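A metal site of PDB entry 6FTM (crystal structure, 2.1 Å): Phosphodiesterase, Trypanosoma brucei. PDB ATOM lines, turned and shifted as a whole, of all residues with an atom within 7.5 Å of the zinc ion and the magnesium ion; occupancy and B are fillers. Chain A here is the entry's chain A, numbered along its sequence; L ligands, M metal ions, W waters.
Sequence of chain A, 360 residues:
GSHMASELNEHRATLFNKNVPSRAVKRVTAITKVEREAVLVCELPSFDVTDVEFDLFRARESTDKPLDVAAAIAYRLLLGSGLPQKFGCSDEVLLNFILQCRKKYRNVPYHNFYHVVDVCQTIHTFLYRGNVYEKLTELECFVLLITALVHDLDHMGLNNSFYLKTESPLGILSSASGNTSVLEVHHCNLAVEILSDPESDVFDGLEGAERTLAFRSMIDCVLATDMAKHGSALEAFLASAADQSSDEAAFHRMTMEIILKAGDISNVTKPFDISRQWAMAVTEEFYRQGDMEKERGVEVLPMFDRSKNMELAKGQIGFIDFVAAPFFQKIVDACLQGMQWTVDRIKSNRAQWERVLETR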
ATOM      1  N   TYR A 110      -0.968  -1.909   1.427  1.00  0.00           N
ATOM      2  CA  TYR A 110      -0.702  -0.964   2.586  1.00  0.00           C
ATOM      3  C   TYR A 110      -1.170   0.501   2.368  1.00  0.00           C
ATOM      4  O   TYR A 110      -1.855   1.114   3.235  1.00  0.00           O
ATOM      5  CB  TYR A 110       0.798  -0.974   2.885  1.00  0.00           C
ATOM      6  CG  TYR A 110       1.204  -0.133   4.101  1.00  0.00           C
ATOM      7  CD1 TYR A 110       1.116  -0.637   5.375  1.00  0.00           C
ATOM      8  CD2 TYR A 110       1.641   1.189   3.953  1.00  0.00           C
ATOM      9  CE1 TYR A 110       1.480   0.149   6.497  1.00  0.00           C
ATOM     10  CE2 TYR A 110       1.990   1.994   5.030  1.00  0.00           C
ATOM     11  CZ  TYR A 110       1.930   1.490   6.308  1.00  0.00           C
ATOM     12  OH  TYR A 110       2.317   2.247   7.368  1.00  0.00           O
ATOM     13  N   HIS A 111      -0.777   1.110   1.257  1.00  0.00           N
ATOM     14  CA  HIS A 111      -1.050   2.566   1.033  1.00  0.00           C
ATOM     15  C   HIS A 111      -2.421   2.869   0.536  1.00  0.00           C
ATOM     16  O   HIS A 111      -2.585   3.515  -0.526  1.00  0.00           O
ATOM     17  CB  HIS A 111       0.012   3.196   0.134  1.00  0.00           C
ATOM     18  CG  HIS A 111       1.331   3.302   0.788  1.00  0.00           C
ATOM     19  ND1 HIS A 111       2.339   2.402   0.540  1.00  0.00           N
ATOM     20  CD2 HIS A 111       1.799   4.169   1.732  1.00  0.00           C
ATOM     21  CE1 HIS A 111       3.384   2.716   1.303  1.00  0.00           C
ATOM     22  NE2 HIS A 111       3.076   3.776   2.040  1.00  0.00           N
ATOM     23  N   HIS A 115      -4.795   3.017   5.824  1.00  0.00           N
ATOM     24  CA  HIS A 115      -3.597   3.734   6.228  1.00  0.00           C
ATOM     25  C   HIS A 115      -3.880   5.186   6.552  1.00  0.00           C
ATOM     26  O   HIS A 115      -3.397   5.631   7.589  1.00  0.00           O
ATOM     27  CB  HIS A 115      -2.490   3.621   5.168  1.00  0.00           C
ATOM     28  CG  HIS A 115      -1.349   4.587   5.337  1.00  0.00           C
ATOM     29  ND1 HIS A 115      -0.461   4.522   6.392  1.00  0.00           N
ATOM     30  CD2 HIS A 115      -0.892   5.577   4.521  1.00  0.00           C
ATOM     31  CE1 HIS A 115       0.461   5.442   6.251  1.00  0.00           C
ATOM     32  NE2 HIS A 115       0.235   6.101   5.117  1.00  0.00           N
ATOM     33  N   VAL A 116      -4.634   5.917   5.706  1.00  0.00           N
ATOM     34  CA  VAL A 116      -4.777   7.333   5.957  1.00  0.00           C
ATOM     35  C   VAL A 116      -5.739   7.659   7.097  1.00  0.00           C
ATOM     36  O   VAL A 116      -5.537   8.671   7.811  1.00  0.00           O
ATOM     37  CB  VAL A 116      -5.054   8.176   4.689  1.00  0.00           C
ATOM     38  CG1 VAL A 116      -3.938   7.896   3.664  1.00  0.00           C
ATOM     39  CG2 VAL A 116      -6.477   7.981   4.111  1.00  0.00           C
ATOM     40  N   VAL A 119      -3.622   7.191  10.134  1.00  0.00           N
ATOM     41  CA  VAL A 119      -2.720   8.349  10.323  1.00  0.00           C
ATOM     42  C   VAL A 119      -3.490   9.522  10.990  1.00  0.00           C
ATOM     43  O   VAL A 119      -2.994  10.200  11.894  1.00  0.00           O
ATOM     44  CB  VAL A 119      -1.971   8.733   8.980  1.00  0.00           C
ATOM     45  CG1 VAL A 119      -1.181  10.044   9.103  1.00  0.00           C
ATOM     46  CG2 VAL A 119      -0.987   7.629   8.556  1.00  0.00           C
ATOM     47  N   ALA A 148      -3.994  14.689   6.823  1.00  0.00           N
ATOM     48  CA  ALA A 148      -3.743  13.242   6.961  1.00  0.00           C
ATOM     49  C   ALA A 148      -4.556  12.429   5.973  1.00  0.00           C
ATOM     50  O   ALA A 148      -4.029  11.431   5.451  1.00  0.00           O
ATOM     51  CB  ALA A 148      -4.005  12.757   8.389  1.00  0.00           C
ATOM     52  N   HIS A 151      -2.970  12.678   2.253  1.00  0.00           N
ATOM     53  CA  HIS A 151      -1.508  12.666   2.130  1.00  0.00           C
ATOM     54  C   HIS A 151      -0.920  11.591   1.194  1.00  0.00           C
ATOM     55  O   HIS A 151       0.226  11.713   0.793  1.00  0.00           O
ATOM     56  CB  HIS A 151      -0.798  12.691   3.520  1.00  0.00           C
ATOM     57  CG  HIS A 151      -0.526  11.333   4.095  1.00  0.00           C
ATOM     58  ND1 HIS A 151      -1.445  10.646   4.845  1.00  0.00           N
ATOM     59  CD2 HIS A 151       0.564  10.525   3.966  1.00  0.00           C
ATOM     60  CE1 HIS A 151      -0.929   9.479   5.172  1.00  0.00           C
ATOM     61  NE2 HIS A 151       0.273   9.362   4.633  1.00  0.00           N
ATOM     62  N   ASP A 152      -1.668  10.530   0.888  1.00  0.00           N
ATOM     63  CA  ASP A 152      -1.209   9.501  -0.051  1.00  0.00           C
ATOM     64  C   ASP A 152      -2.206   9.195  -1.188  1.00  0.00           C
ATOM     65  O   ASP A 152      -2.202   8.085  -1.703  1.00  0.00           O
ATOM     66  CB  ASP A 152      -0.935   8.174   0.708  1.00  0.00           C
ATOM     67  CG  ASP A 152       0.456   8.078   1.357  1.00  0.00           C
ATOM     68  OD1 ASP A 152       1.461   8.645   0.891  1.00  0.00           O
ATOM     69  OD2 ASP A 152       0.487   7.336   2.352  1.00  0.00           O
ATOM     70  N   LEU A 153      -2.977  10.196  -1.624  1.00  0.00           N
ATOM     71  CA  LEU A 153      -4.044  10.001  -2.632  1.00  0.00           C
ATOM     72  C   LEU A 153      -3.511   9.320  -3.918  1.00  0.00           C
ATOM     73  O   LEU A 153      -2.519   9.774  -4.488  1.00  0.00           O
ATOM     74  CB  LEU A 153      -4.709  11.340  -2.962  1.00  0.00           C
ATOM     75  CG  LEU A 153      -5.758  11.951  -2.006  1.00  0.00           C
ATOM     76  CD1 LEU A 153      -6.003  13.412  -2.280  1.00  0.00           C
ATOM     77  CD2 LEU A 153      -7.147  11.314  -2.037  1.00  0.00           C
ATOM     78  N   HIS A 155      -2.029   6.481  -4.377  1.00  0.00           N
ATOM     79  CA  HIS A 155      -0.742   5.707  -4.241  1.00  0.00           C
ATOM     80  C   HIS A 155      -0.946   4.297  -4.895  1.00  0.00           C
ATOM     81  O   HIS A 155      -1.952   3.616  -4.619  1.00  0.00           O
ATOM     82  CB  HIS A 155      -0.383   5.526  -2.748  1.00  0.00           C
ATOM     83  CG  HIS A 155       1.078   5.304  -2.433  1.00  0.00           C
ATOM     84  ND1 HIS A 155       1.812   4.190  -2.854  1.00  0.00           N
ATOM     85  CD2 HIS A 155       1.928   6.048  -1.650  1.00  0.00           C
ATOM     86  CE1 HIS A 155       3.056   4.283  -2.370  1.00  0.00           C
ATOM     87  NE2 HIS A 155       3.159   5.431  -1.664  1.00  0.00           N
ATOM     88  N   LEU A 183       5.670  10.939  -6.210  1.00  0.00           N
ATOM     89  CA  LEU A 183       4.468  10.590  -5.479  1.00  0.00           C
ATOM     90  C   LEU A 183       3.839  11.744  -4.749  1.00  0.00           C
ATOM     91  O   LEU A 183       2.624  11.952  -4.891  1.00  0.00           O
ATOM     92  CB  LEU A 183       4.740   9.499  -4.467  1.00  0.00           C
ATOM     93  CG  LEU A 183       4.709   8.031  -4.893  1.00  0.00           C
ATOM     94  CD1 LEU A 183       5.476   7.198  -3.890  1.00  0.00           C
ATOM     95  CD2 LEU A 183       3.263   7.583  -4.927  1.00  0.00           C
ATOM     96  N   GLU A 184       4.654  12.505  -4.021  1.00  0.00           N
ATOM     97  CA  GLU A 184       4.115  13.554  -3.129  1.00  0.00           C
ATOM     98  C   GLU A 184       3.514  14.724  -3.944  1.00  0.00           C
ATOM     99  O   GLU A 184       2.469  15.270  -3.593  1.00  0.00           O
ATOM    100  CB  GLU A 184       5.142  13.970  -2.042  1.00  0.00           C
ATOM    101  CG  GLU A 184       5.527  12.811  -1.076  1.00  0.00           C
ATOM    102  CD  GLU A 184       6.430  11.672  -1.673  1.00  0.00           C
ATOM    103  OE1 GLU A 184       7.077  11.933  -2.766  1.00  0.00           O
ATOM    104  OE2 GLU A 184       6.470  10.528  -1.074  1.00  0.00           O
ATOM    105  N   HIS A 187       0.026  13.458  -5.057  1.00  0.00           N
ATOM    106  CA  HIS A 187      -0.950  13.501  -3.966  1.00  0.00           C
ATOM    107  C   HIS A 187      -1.461  14.941  -3.797  1.00  0.00           C
ATOM    108  O   HIS A 187      -2.640  15.147  -3.606  1.00  0.00           O
ATOM    109  CB  HIS A 187      -0.425  12.991  -2.585  1.00  0.00           C
ATOM    110  CG  HIS A 187       0.290  11.661  -2.591  1.00  0.00           C
ATOM    111  ND1 HIS A 187      -0.176  10.536  -3.267  1.00  0.00           N
ATOM    112  CD2 HIS A 187       1.467  11.310  -1.998  1.00  0.00           C
ATOM    113  CE1 HIS A 187       0.688   9.537  -3.071  1.00  0.00           C
ATOM    114  NE2 HIS A 187       1.691   9.978  -2.306  1.00  0.00           N
ATOM    115  N   VAL A 222       2.600  17.598   3.033  1.00  0.00           N
ATOM    116  CA  VAL A 222       2.590  16.452   2.125  1.00  0.00           C
ATOM    117  C   VAL A 222       3.974  16.253   1.465  1.00  0.00           C
ATOM    118  O   VAL A 222       4.482  15.192   1.463  1.00  0.00           O
ATOM    119  CB  VAL A 222       1.458  16.500   1.083  1.00  0.00           C
ATOM    120  CG1 VAL A 222       1.554  15.377   0.088  1.00  0.00           C
ATOM    121  CG2 VAL A 222       0.082  16.552   1.734  1.00  0.00           C
ATOM    122  N   THR A 225       6.564  14.467   3.573  1.00  0.00           N
ATOM    123  CA  THR A 225       6.424  13.041   3.840  1.00  0.00           C
ATOM    124  C   THR A 225       7.338  12.128   2.972  1.00  0.00           C
ATOM    125  O   THR A 225       7.360  10.890   3.157  1.00  0.00           O
ATOM    126  CB  THR A 225       4.983  12.520   3.768  1.00  0.00           C
ATOM    127  OG1 THR A 225       4.377  12.708   2.452  1.00  0.00           O
ATOM    128  CG2 THR A 225       4.133  13.215   4.833  1.00  0.00           C
ATOM    129  N   ASP A 226       8.024  12.692   2.007  1.00  0.00           N
ATOM    130  CA  ASP A 226       8.946  11.933   1.134  1.00  0.00           C
ATOM    131  C   ASP A 226      10.150  11.568   1.980  1.00  0.00           C
ATOM    132  O   ASP A 226      10.820  12.462   2.530  1.00  0.00           O
ATOM    133  CB  ASP A 226       9.357  12.824  -0.047  1.00  0.00           C
ATOM    134  CG  ASP A 226      10.479  12.157  -0.968  1.00  0.00           C
ATOM    135  OD1 ASP A 226      10.956  11.090  -0.624  1.00  0.00           O
ATOM    136  OD2 ASP A 226      10.812  12.726  -2.010  1.00  0.00           O
ATOM    137  N   MET A 227      10.403  10.276   2.154  1.00  0.00           N
ATOM    138  CA  MET A 227      11.501   9.865   3.042  1.00  0.00           C
ATOM    139  C   MET A 227      12.909  10.298   2.607  1.00  0.00           C
ATOM    140  O   MET A 227      13.828  10.370   3.450  1.00  0.00           O
ATOM    141  CB  MET A 227      11.492   8.383   3.389  1.00  0.00           C
ATOM    142  CG  MET A 227      10.425   7.985   4.414  1.00  0.00           C
ATOM    143  SD  MET A 227      10.503   8.713   6.067  1.00  0.00           S
ATOM    144  CE  MET A 227      11.819   7.713   6.739  1.00  0.00           C
ATOM    145  N   LEU A 260       2.957  15.257  11.059  1.00  0.00           N
ATOM    146  CA  LEU A 260       2.462  14.389   9.956  1.00  0.00           C
ATOM    147  C   LEU A 260       3.412  13.213   9.717  1.00  0.00           C
ATOM    148  O   LEU A 260       2.970  12.065   9.556  1.00  0.00           O
ATOM    149  CB  LEU A 260       2.264  15.174   8.641  1.00  0.00           C
ATOM    150  CG  LEU A 260       1.759  14.304   7.455  1.00  0.00           C
ATOM    151  CD1 LEU A 260       0.450  13.609   7.750  1.00  0.00           C
ATOM    152  CD2 LEU A 260       1.567  15.137   6.240  1.00  0.00           C
ATOM    153  N   GLY A 263       2.912  10.612  12.612  1.00  0.00           N
ATOM    154  CA  GLY A 263       1.737   9.769  12.285  1.00  0.00           C
ATOM    155  C   GLY A 263       2.029   8.743  11.179  1.00  0.00           C
ATOM    156  O   GLY A 263       1.656   7.571  11.279  1.00  0.00           O
ATOM    157  N   ASP A 264       2.712   9.204  10.139  1.00  0.00           N
ATOM    158  CA  ASP A 264       3.047   8.368   8.978  1.00  0.00           C
ATOM    159  C   ASP A 264       3.871   7.136   9.302  1.00  0.00           C
ATOM    160  O   ASP A 264       3.637   6.075   8.701  1.00  0.00           O
ATOM    161  CB  ASP A 264       3.746   9.186   7.876  1.00  0.00           C
ATOM    162  CG  ASP A 264       3.487   8.629   6.437  1.00  0.00           C
ATOM    163  OD1 ASP A 264       2.472   7.910   6.239  1.00  0.00           O
ATOM    164  OD2 ASP A 264       4.334   8.875   5.541  1.00  0.00           O
ATOM    165  N   ILE A 265       4.818   7.244  10.242  1.00  0.00           N
ATOM    166  CA  ILE A 265       5.605   6.064  10.672  1.00  0.00           C
ATOM    167  C   ILE A 265       5.249   5.575  12.110  1.00  0.00           C
ATOM    168  O   ILE A 265       6.103   4.999  12.816  1.00  0.00           O
ATOM    169  CB  ILE A 265       7.112   6.308  10.580  1.00  0.00           C
ATOM    170  CG1 ILE A 265       7.539   7.463  11.473  1.00  0.00           C
ATOM    171  CG2 ILE A 265       7.500   6.633   9.119  1.00  0.00           C
ATOM    172  CD1 ILE A 265       9.040   7.603  11.565  1.00  0.00           C
HETATM  173  C1  LIG L   1       6.055  -0.844   9.734  1.00  0.00           C
HETATM  174  C2  LIG L   1      10.640  -3.854   7.332  1.00  0.00           C
HETATM  175  C3  LIG L   1       8.869   2.900   5.208  1.00  0.00           C
HETATM  176  C4  LIG L   1      11.991   3.787   3.671  1.00  0.00           C
HETATM  177  C5  LIG L   1      12.434   2.415   3.139  1.00  0.00           C
HETATM  178  C6  LIG L   1      13.787   2.352   2.444  1.00  0.00           C
HETATM  179  C7  LIG L   1      14.885   2.581   3.431  1.00  0.00           C
HETATM  180  C8  LIG L   1      15.051   4.011   3.814  1.00  0.00           C
HETATM  181  C9  LIG L   1      14.178   4.495   4.936  1.00  0.00           C
HETATM  182  C10 LIG L   1      12.683   4.195   4.942  1.00  0.00           C
HETATM  183  C11 LIG L   1       9.667   4.500   3.051  1.00  0.00           C
HETATM  184  C12 LIG L   1       7.588  -0.032   8.066  1.00  0.00           C
HETATM  185  C13 LIG L   1       8.187   4.240   3.204  1.00  0.00           C
HETATM  186  C14 LIG L   1       7.303   5.358   2.607  1.00  0.00           C
HETATM  187  C15 LIG L   1       7.116   6.507   3.537  1.00  0.00           C
HETATM  188  C16 LIG L   1       7.419   6.481   4.829  1.00  0.00           C
HETATM  189  C17 LIG L   1       8.002   5.288   5.522  1.00  0.00           C
HETATM  190  C18 LIG L   1       7.895   3.971   4.693  1.00  0.00           C
HETATM  191  C19 LIG L   1       6.885   1.144   7.895  1.00  0.00           C
HETATM  192  C20 LIG L   1       7.295   2.082   6.961  1.00  0.00           C
HETATM  193  C21 LIG L   1       8.431   1.871   6.186  1.00  0.00           C
HETATM  194  C22 LIG L   1       9.150   0.682   6.349  1.00  0.00           C
HETATM  195  C23 LIG L   1       8.747  -0.278   7.282  1.00  0.00           C
HETATM  196  C24 LIG L   1       9.473  -1.512   7.399  1.00  0.00           C
HETATM  197  C25 LIG L   1      10.050  -2.563   7.405  1.00  0.00           C
HETATM  198  N1  LIG L   1      11.619  -4.078   6.412  1.00  0.00           N
HETATM  199  N2  LIG L   1      10.099   2.866   4.820  1.00  0.00           N
HETATM  200  N3  LIG L   1      10.525   3.758   3.872  1.00  0.00           N
HETATM  201  O1  LIG L   1       7.243  -1.019   8.949  1.00  0.00           O
HETATM  202  O2  LIG L   1      10.239  -4.669   8.151  1.00  0.00           O
HETATM  203  O3  LIG L   1      10.095   5.305   2.239  1.00  0.00           O
HETATM  204 ZN    ZN M   1       1.603   7.599   4.284  1.00  0.00          ZN
HETATM  205 MG    MG M   2       3.489   8.907   1.242  1.00  0.00          MG
HETATM  206  O   HOH W   1       3.255   6.050   3.929  1.00  0.00           O
HETATM  207  O   HOH W   2       3.857   8.985  -0.813  1.00  0.00           O
HETATM  208  O   HOH W   3       3.115   8.801   3.192  1.00  0.00           O
HETATM  209  O   HOH W   4       5.552   9.509   1.509  1.00  0.00           O
HETATM  210  O   HOH W   5       2.917  10.784   1.106  1.00  0.00           O
HETATM  211  O   HOH W   6       4.040   6.934   1.328  1.00  0.00           O
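ND1 of His 151 lies within hydrogen-bond range of O of Ala 148, at 2.8 Å.
NE2 of His 187 sits close to OD1 of Asp 152 (3.5 Å).
Four residues have an atom within 4 Å of the zinc ion: His 115, His 151, Asp 152 and Asp 264.
The nearest printed residue that does not touch the zinc ion is His 111 (4.3 Å).
One residue has an atom within 4 Å of the magnesium ion: Asp 152.
The zinc ion is bound by OD1 of Asp 264 (2.2 Å), NE2 of His 115 (2.2 Å), water W3 (2.2 Å), NE2 of His 151 (2.2 Å), OD2 of Asp 152 (2.2 Å) and water W1 (2.3 Å).
The magnesium ion is bound by water W5 (2.0 Å), water W3 (2.0 Å), water W6 (2.1 Å), OD1 of Asp 152 (2.1 Å), water W2 (2.1 Å) and water W4 (2.2 Å).
The magnesium ion has six donor atoms within binding distance.
Water W1 lies within hydrogen-bond range of NE2 of His 111 and OD2 of Asp 264.
Water W4 bridges O of Thr 225 (2.8 Å) and OE2 of Glu 184 (2.9 Å).
Water W2 lies within hydrogen-bond range of a ring nitrogen (NE2) of His 187 and the side-chain carboxylate of Glu 184.
Water W6 bridges a ring nitrogen (NE2) of His 111 (3.4 Å) and a ring nitrogen (NE2) of His 155 (3.5 Å).
Water W5 lies within hydrogen-bond range of the side-chain hydroxyl of Thr 225 and the backbone carbonyl oxygen of His 151.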
